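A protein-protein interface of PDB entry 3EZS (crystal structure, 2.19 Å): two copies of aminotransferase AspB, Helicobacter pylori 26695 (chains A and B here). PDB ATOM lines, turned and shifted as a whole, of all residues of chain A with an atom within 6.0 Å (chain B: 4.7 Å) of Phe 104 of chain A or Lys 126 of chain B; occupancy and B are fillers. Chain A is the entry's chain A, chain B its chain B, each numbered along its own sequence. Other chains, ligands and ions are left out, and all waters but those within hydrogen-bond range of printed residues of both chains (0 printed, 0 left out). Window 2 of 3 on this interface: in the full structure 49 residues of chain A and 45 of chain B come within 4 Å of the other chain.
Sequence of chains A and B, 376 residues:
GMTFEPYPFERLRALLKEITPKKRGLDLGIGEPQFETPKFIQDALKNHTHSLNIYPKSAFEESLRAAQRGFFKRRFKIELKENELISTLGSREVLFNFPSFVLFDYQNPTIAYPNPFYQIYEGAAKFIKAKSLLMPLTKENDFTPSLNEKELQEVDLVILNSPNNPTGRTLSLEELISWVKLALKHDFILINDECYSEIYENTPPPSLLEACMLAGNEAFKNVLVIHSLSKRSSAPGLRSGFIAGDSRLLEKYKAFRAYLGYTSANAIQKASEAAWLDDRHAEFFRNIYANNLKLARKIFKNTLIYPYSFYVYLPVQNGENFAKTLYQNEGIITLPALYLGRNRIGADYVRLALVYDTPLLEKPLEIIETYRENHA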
ATOM      1  N   PRO A  99       5.477   7.938  12.976  1.00  0.00           N
ATOM      2  CA  PRO A  99       5.022   8.471  14.276  1.00  0.00           C
ATOM      3  C   PRO A  99       4.722   9.984  14.278  1.00  0.00           C
ATOM      4  O   PRO A  99       3.766  10.391  14.930  1.00  0.00           O
ATOM      5  CB  PRO A  99       6.182   8.134  15.217  1.00  0.00           C
ATOM      6  CG  PRO A  99       6.907   6.946  14.528  1.00  0.00           C
ATOM      7  CD  PRO A  99       6.797   7.285  13.074  1.00  0.00           C
ATOM      8  N   SER A 100       5.511  10.804  13.568  1.00  0.00           N
ATOM      9  CA  SER A 100       5.218  12.243  13.505  1.00  0.00           C
ATOM     10  C   SER A 100       3.909  12.476  12.743  1.00  0.00           C
ATOM     11  O   SER A 100       3.186  13.426  13.018  1.00  0.00           O
ATOM     12  CB  SER A 100       6.371  13.078  12.894  1.00  0.00           C
ATOM     13  OG  SER A 100       6.574  12.825  11.512  1.00  0.00           O
ATOM     14  N   PHE A 101       3.609  11.621  11.777  1.00  0.00           N
ATOM     15  CA  PHE A 101       2.334  11.709  11.097  1.00  0.00           C
ATOM     16  C   PHE A 101       1.170  11.369  12.048  1.00  0.00           C
ATOM     17  O   PHE A 101       0.293  12.197  12.247  1.00  0.00           O
ATOM     18  CB  PHE A 101       2.305  10.815   9.859  1.00  0.00           C
ATOM     19  CG  PHE A 101       0.912  10.417   9.435  1.00  0.00           C
ATOM     20  CD1 PHE A 101       0.068  11.329   8.810  1.00  0.00           C
ATOM     21  CD2 PHE A 101       0.442   9.126   9.679  1.00  0.00           C
ATOM     22  CE1 PHE A 101      -1.227  10.954   8.443  1.00  0.00           C
ATOM     23  CE2 PHE A 101      -0.844   8.752   9.314  1.00  0.00           C
ATOM     24  CZ  PHE A 101      -1.673   9.664   8.690  1.00  0.00           C
ATOM     25  N   VAL A 102       1.187  10.171  12.643  1.00  0.00           N
ATOM     26  CA  VAL A 102       0.070   9.717  13.486  1.00  0.00           C
ATOM     27  C   VAL A 102      -0.112  10.491  14.768  1.00  0.00           C
ATOM     28  O   VAL A 102      -1.246  10.683  15.196  1.00  0.00           O
ATOM     29  CB  VAL A 102       0.117   8.193  13.861  1.00  0.00           C
ATOM     30  CG1 VAL A 102      -0.116   7.371  12.665  1.00  0.00           C
ATOM     31  CG2 VAL A 102       1.411   7.816  14.546  1.00  0.00           C
ATOM     32  N   LEU A 103       0.984  10.957  15.357  1.00  0.00           N
ATOM     33  CA  LEU A 103       0.912  11.700  16.619  1.00  0.00           C
ATOM     34  C   LEU A 103       1.002  13.210  16.400  1.00  0.00           C
ATOM     35  O   LEU A 103       1.183  13.958  17.344  1.00  0.00           O
ATOM     36  CB  LEU A 103       2.009  11.202  17.581  1.00  0.00           C
ATOM     37  CG  LEU A 103       2.051   9.676  17.809  1.00  0.00           C
ATOM     38  CD1 LEU A 103       3.232   9.229  18.686  1.00  0.00           C
ATOM     39  CD2 LEU A 103       0.741   9.167  18.402  1.00  0.00           C
ATOM     40  N   PHE A 104       0.789  13.647  15.161  1.00  0.00           N
ATOM     41  CA  PHE A 104       0.987  15.040  14.771  1.00  0.00           C
ATOM     42  C   PHE A 104       0.354  16.090  15.667  1.00  0.00           C
ATOM     43  O   PHE A 104       0.987  17.116  15.970  1.00  0.00           O
ATOM     44  CB  PHE A 104       0.505  15.283  13.328  1.00  0.00           C
ATOM     45  CG  PHE A 104       0.815  16.659  12.831  1.00  0.00           C
ATOM     46  CD1 PHE A 104       2.114  17.008  12.508  1.00  0.00           C
ATOM     47  CD2 PHE A 104      -0.173  17.616  12.724  1.00  0.00           C
ATOM     48  CE1 PHE A 104       2.416  18.288  12.057  1.00  0.00           C
ATOM     49  CE2 PHE A 104       0.124  18.891  12.287  1.00  0.00           C
ATOM     50  CZ  PHE A 104       1.415  19.224  11.959  1.00  0.00           C
ATOM     51  N   ASP A 105      -0.894  15.864  16.062  1.00  0.00           N
ATOM     52  CA  ASP A 105      -1.588  16.839  16.902  1.00  0.00           C
ATOM     53  C   ASP A 105      -1.687  16.446  18.385  1.00  0.00           C
ATOM     54  O   ASP A 105      -2.436  17.072  19.140  1.00  0.00           O
ATOM     55  CB  ASP A 105      -2.973  17.092  16.316  1.00  0.00           C
ATOM     56  CG  ASP A 105      -2.924  17.935  15.046  1.00  0.00           C
ATOM     57  OD1 ASP A 105      -2.348  19.064  15.088  1.00  0.00           O
ATOM     58  OD2 ASP A 105      -3.495  17.476  14.021  1.00  0.00           O
ATOM     59  N   TYR A 106      -0.920  15.439  18.817  1.00  0.00           N
ATOM     60  CA  TYR A 106      -1.002  15.000  20.205  1.00  0.00           C
ATOM     61  C   TYR A 106      -0.192  15.878  21.115  1.00  0.00           C
ATOM     62  O   TYR A 106       0.918  16.282  20.774  1.00  0.00           O
ATOM     63  CB  TYR A 106      -0.476  13.596  20.391  1.00  0.00           C
ATOM     64  CG  TYR A 106      -1.373  12.462  19.959  1.00  0.00           C
ATOM     65  CD1 TYR A 106      -1.894  12.401  18.664  1.00  0.00           C
ATOM     66  CD2 TYR A 106      -1.604  11.388  20.816  1.00  0.00           C
ATOM     67  CE1 TYR A 106      -2.668  11.320  18.257  1.00  0.00           C
ATOM     68  CE2 TYR A 106      -2.356  10.303  20.419  1.00  0.00           C
ATOM     69  CZ  TYR A 106      -2.892  10.268  19.143  1.00  0.00           C
ATOM     70  OH  TYR A 106      -3.646   9.177  18.757  1.00  0.00           O
ATOM     71  N   ILE A 128       9.206  13.943  17.156  1.00  0.00           N
ATOM     72  CA  ILE A 128       7.837  14.354  17.517  1.00  0.00           C
ATOM     73  C   ILE A 128       7.770  14.740  19.020  1.00  0.00           C
ATOM     74  O   ILE A 128       6.699  14.903  19.581  1.00  0.00           O
ATOM     75  CB  ILE A 128       6.788  13.255  17.089  1.00  0.00           C
ATOM     76  CG1 ILE A 128       5.334  13.776  17.131  1.00  0.00           C
ATOM     77  CG2 ILE A 128       6.958  11.963  17.935  1.00  0.00           C
ATOM     78  CD1 ILE A 128       5.040  15.057  16.303  1.00  0.00           C
ATOM     79  N   TYR A 259       3.693  15.240   0.099  1.00  0.00           N
ATOM     80  CA  TYR A 259       4.595  16.360   0.385  1.00  0.00           C
ATOM     81  C   TYR A 259       6.069  16.029   0.676  1.00  0.00           C
ATOM     82  O   TYR A 259       6.929  16.911   0.596  1.00  0.00           O
ATOM     83  CB  TYR A 259       4.085  17.086   1.636  1.00  0.00           C
ATOM     84  CG  TYR A 259       2.719  17.694   1.497  1.00  0.00           C
ATOM     85  CD1 TYR A 259       2.557  18.979   0.970  1.00  0.00           C
ATOM     86  CD2 TYR A 259       1.587  16.990   1.886  1.00  0.00           C
ATOM     87  CE1 TYR A 259       1.296  19.548   0.838  1.00  0.00           C
ATOM     88  CE2 TYR A 259       0.317  17.543   1.766  1.00  0.00           C
ATOM     89  CZ  TYR A 259       0.170  18.825   1.244  1.00  0.00           C
ATOM     90  OH  TYR A 259      -1.100  19.375   1.110  1.00  0.00           O
ATOM     91  N   MET B   2      -4.092  17.350  11.380  1.00  0.00           N
ATOM     92  CA  MET B   2      -3.336  17.556  10.109  1.00  0.00           C
ATOM     93  C   MET B   2      -4.309  17.779   8.947  1.00  0.00           C
ATOM     94  O   MET B   2      -5.144  16.908   8.669  1.00  0.00           O
ATOM     95  CB  MET B   2      -2.418  16.358   9.821  1.00  0.00           C
ATOM     96  CG  MET B   2      -1.665  16.503   8.507  1.00  0.00           C
ATOM     97  SD  MET B   2      -0.154  15.311   8.156  1.00  0.00           S
ATOM     98  CE  MET B   2       1.125  15.933   9.488  1.00  0.00           C
ATOM     99  N   THR B   3      -4.189  18.930   8.271  1.00  0.00           N
ATOM    100  CA  THR B   3      -5.089  19.307   7.156  1.00  0.00           C
ATOM    101  C   THR B   3      -4.398  19.264   5.791  1.00  0.00           C
ATOM    102  O   THR B   3      -3.259  19.716   5.648  1.00  0.00           O
ATOM    103  CB  THR B   3      -5.681  20.718   7.372  1.00  0.00           C
ATOM    104  OG1 THR B   3      -6.563  20.695   8.503  1.00  0.00           O
ATOM    105  CG2 THR B   3      -6.459  21.175   6.144  1.00  0.00           C
ATOM    106  N   PHE B   4      -5.104  18.741   4.787  1.00  0.00           N
ATOM    107  CA  PHE B   4      -4.542  18.598   3.433  1.00  0.00           C
ATOM    108  C   PHE B   4      -5.231  19.499   2.396  1.00  0.00           C
ATOM    109  O   PHE B   4      -6.412  19.327   2.090  1.00  0.00           O
ATOM    110  CB  PHE B   4      -4.584  17.123   3.008  1.00  0.00           C
ATOM    111  CG  PHE B   4      -3.966  16.188   4.023  1.00  0.00           C
ATOM    112  CD1 PHE B   4      -2.588  16.152   4.205  1.00  0.00           C
ATOM    113  CD2 PHE B   4      -4.761  15.354   4.804  1.00  0.00           C
ATOM    114  CE1 PHE B   4      -2.010  15.299   5.142  1.00  0.00           C
ATOM    115  CE2 PHE B   4      -4.186  14.491   5.747  1.00  0.00           C
ATOM    116  CZ  PHE B   4      -2.815  14.463   5.912  1.00  0.00           C
ATOM    117  N   GLU B   5      -4.480  20.474   1.880  1.00  0.00           N
ATOM    118  CA  GLU B   5      -4.983  21.387   0.859  1.00  0.00           C
ATOM    119  C   GLU B   5      -4.892  20.669  -0.490  1.00  0.00           C
ATOM    120  O   GLU B   5      -3.850  20.084  -0.799  1.00  0.00           O
ATOM    121  CB  GLU B   5      -4.161  22.687   0.814  1.00  0.00           C
ATOM    122  N   GLU B 122       3.962  25.909   1.235  1.00  0.00           N
ATOM    123  CA  GLU B 122       2.893  25.944   2.248  1.00  0.00           C
ATOM    124  C   GLU B 122       2.857  24.658   3.083  1.00  0.00           C
ATOM    125  O   GLU B 122       2.657  24.692   4.302  1.00  0.00           O
ATOM    126  CB  GLU B 122       1.527  26.198   1.619  1.00  0.00           C
ATOM    127  CG  GLU B 122       0.460  26.468   2.636  1.00  0.00           C
ATOM    128  CD  GLU B 122      -0.889  26.694   2.024  1.00  0.00           C
ATOM    129  OE1 GLU B 122      -1.536  25.693   1.669  1.00  0.00           O
ATOM    130  OE2 GLU B 122      -1.318  27.867   1.949  1.00  0.00           O
ATOM    131  N   GLY B 123       3.027  23.524   2.425  1.00  0.00           N
ATOM    132  CA  GLY B 123       3.077  22.246   3.132  1.00  0.00           C
ATOM    133  C   GLY B 123       4.153  22.254   4.206  1.00  0.00           C
ATOM    134  O   GLY B 123       3.921  21.823   5.339  1.00  0.00           O
ATOM    135  N   ALA B 124       5.314  22.805   3.851  1.00  0.00           N
ATOM    136  CA  ALA B 124       6.470  22.881   4.746  1.00  0.00           C
ATOM    137  C   ALA B 124       6.176  23.731   5.959  1.00  0.00           C
ATOM    138  O   ALA B 124       6.526  23.364   7.077  1.00  0.00           O
ATOM    139  CB  ALA B 124       7.683  23.423   3.987  1.00  0.00           C
ATOM    140  N   ALA B 125       5.512  24.864   5.734  1.00  0.00           N
ATOM    141  CA  ALA B 125       5.113  25.775   6.800  1.00  0.00           C
ATOM    142  C   ALA B 125       4.104  25.130   7.737  1.00  0.00           C
ATOM    143  O   ALA B 125       4.238  25.248   8.958  1.00  0.00           O
ATOM    144  CB  ALA B 125       4.542  27.053   6.213  1.00  0.00           C
ATOM    145  N   LYS B 126       3.086  24.468   7.175  1.00  0.00           N
ATOM    146  CA  LYS B 126       2.066  23.791   7.997  1.00  0.00           C
ATOM    147  C   LYS B 126       2.663  22.677   8.851  1.00  0.00           C
ATOM    148  O   LYS B 126       2.322  22.545  10.009  1.00  0.00           O
ATOM    149  CB  LYS B 126       0.916  23.248   7.143  1.00  0.00           C
ATOM    150  CG  LYS B 126       0.034  24.343   6.518  1.00  0.00           C
ATOM    151  CD  LYS B 126      -0.884  23.825   5.392  1.00  0.00           C
ATOM    152  CE  LYS B 126      -2.121  23.126   5.898  1.00  0.00           C
ATOM    153  NZ  LYS B 126      -2.956  22.566   4.783  1.00  0.00           N
ATOM    154  N   PHE B 127       3.577  21.898   8.292  1.00  0.00           N
ATOM    155  CA  PHE B 127       4.186  20.823   9.046  1.00  0.00           C
ATOM    156  C   PHE B 127       4.901  21.335  10.304  1.00  0.00           C
ATOM    157  O   PHE B 127       4.741  20.757  11.371  1.00  0.00           O
ATOM    158  CB  PHE B 127       5.124  20.024   8.151  1.00  0.00           C
ATOM    159  CG  PHE B 127       5.680  18.788   8.799  1.00  0.00           C
ATOM    160  CD1 PHE B 127       4.838  17.847   9.386  1.00  0.00           C
ATOM    161  CD2 PHE B 127       7.046  18.526   8.749  1.00  0.00           C
ATOM    162  CE1 PHE B 127       5.358  16.683   9.982  1.00  0.00           C
ATOM    163  CE2 PHE B 127       7.579  17.369   9.323  1.00  0.00           C
ATOM    164  CZ  PHE B 127       6.730  16.443   9.939  1.00  0.00           C
ATOM    165  N   ILE B 128       5.637  22.444  10.194  1.00  0.00           N
ATOM    166  CA  ILE B 128       6.327  23.025  11.345  1.00  0.00           C
ATOM    167  C   ILE B 128       5.411  23.976  12.139  1.00  0.00           C
ATOM    168  O   ILE B 128       5.863  24.650  13.048  1.00  0.00           O
ATOM    169  CB  ILE B 128       7.706  23.668  10.931  1.00  0.00           C
ATOM    170  CG1 ILE B 128       8.609  23.968  12.148  1.00  0.00           C
ATOM    171  CG2 ILE B 128       7.527  24.938  10.073  1.00  0.00           C
ATOM    172  CD1 ILE B 128       8.877  22.797  13.086  1.00  0.00           C
ATOM    173  N   LYS B 129       4.116  23.989  11.826  1.00  0.00           N
ATOM    174  CA  LYS B 129       3.125  24.848  12.507  1.00  0.00           C
ATOM    175  C   LYS B 129       3.495  26.342  12.494  1.00  0.00           C
ATOM    176  O   LYS B 129       3.279  27.052  13.460  1.00  0.00           O
ATOM    177  CB  LYS B 129       2.882  24.340  13.943  1.00  0.00           C
ATOM    178  CG  LYS B 129       2.503  22.836  14.005  1.00  0.00           C
ATOM    179  CD  LYS B 129       2.307  22.311  15.432  1.00  0.00           C
ATOM    180  CE  LYS B 129       2.275  20.774  15.466  1.00  0.00           C
ATOM    181  NZ  LYS B 129       2.127  20.218  16.850  1.00  0.00           N
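Printed residues of chain B that touch a printed residue of chain A: Met 2, Glu 5, Gly 123, Lys 126, Phe 127 and Lys 129.
Hydrophobic or aromatic side chains of chain B within 4 Å of the printed part of chain A: Met 2 and Phe 127.
Hydrophobic or aromatic side chains of chain A that line the printed part of chain B: Phe 104 and Tyr 259.
Among the printed residues, 8 pairs touch across the chains.
Among the printed residues, merely in contact across the chains: Phe 104 of chain A with Met 2 of chain B, Phe 104 of chain A with Phe 127 of chain B, Ser 100 of chain A with Phe 127 of chain B, Tyr 259 of chain A with Gly 123 of chain B and Phe 104 of chain A with Lys 126 of chain B.
Printed residues of chain B within 4 Å of Phe 104 of chain A: Met 2 (3.4 Å), Lys 126 (3.96 Å), Phe 127 (3.5 Å) and Lys 129 (3.4 Å).
Lys 126 of chain B touches just one residue of chain A: Phe 104.
Printed residues of chain A within 4 Å of Gly 123 of chain B: Tyr 259.
Of the printed residues of chain A, Lys 129 of chain B touches Phe 104.
Printed residues of chain B within 4 Å of Tyr 259 of chain A: Glu 5 and Gly 123.
Printed residues of chain A within 4 Å of Glu 5 of chain B: Tyr 259 (3.4 Å).
Printed residues of chain A within 4 Å of Phe 127 of chain B: Ser 100 and Phe 104.
The nearest printed residue of chain B that does not touch Phe 104 of chain A is Ile 128 of chain B (5.6 Å).
The nearest residue of chain A that does not touch Lys 126 of chain B is Tyr 259 of chain A (5.2 Å).
The nearest printed residue of chain A that does not touch Glu 5 of chain B is Phe 104 of chain A (11.5 Å).
The backbone carbonyl oxygen (O) of Thr 3 of chain B is in hydrogen-bond range of the side-chain amino group (NZ) of Lys 126 of chain B (3.0 Å).
Position printed for both chains: 128.
The backbone carbonyl oxygen (O) of Phe 104 of chain A lies within hydrogen-bond range of the side-chain amino group (NZ) of Lys 129 of chain B (3.4 Å).
OD2 of Asp 105 of chain A sits at hydrogen-bond distance from N of Met 2 of chain B, 2.7 Å away.
The side-chain hydroxyl (OH) of Tyr 259 of chain A sits at hydrogen-bond distance from the backbone carbonyl oxygen (O) of Glu 5 of chain B, at 3.4 Å.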
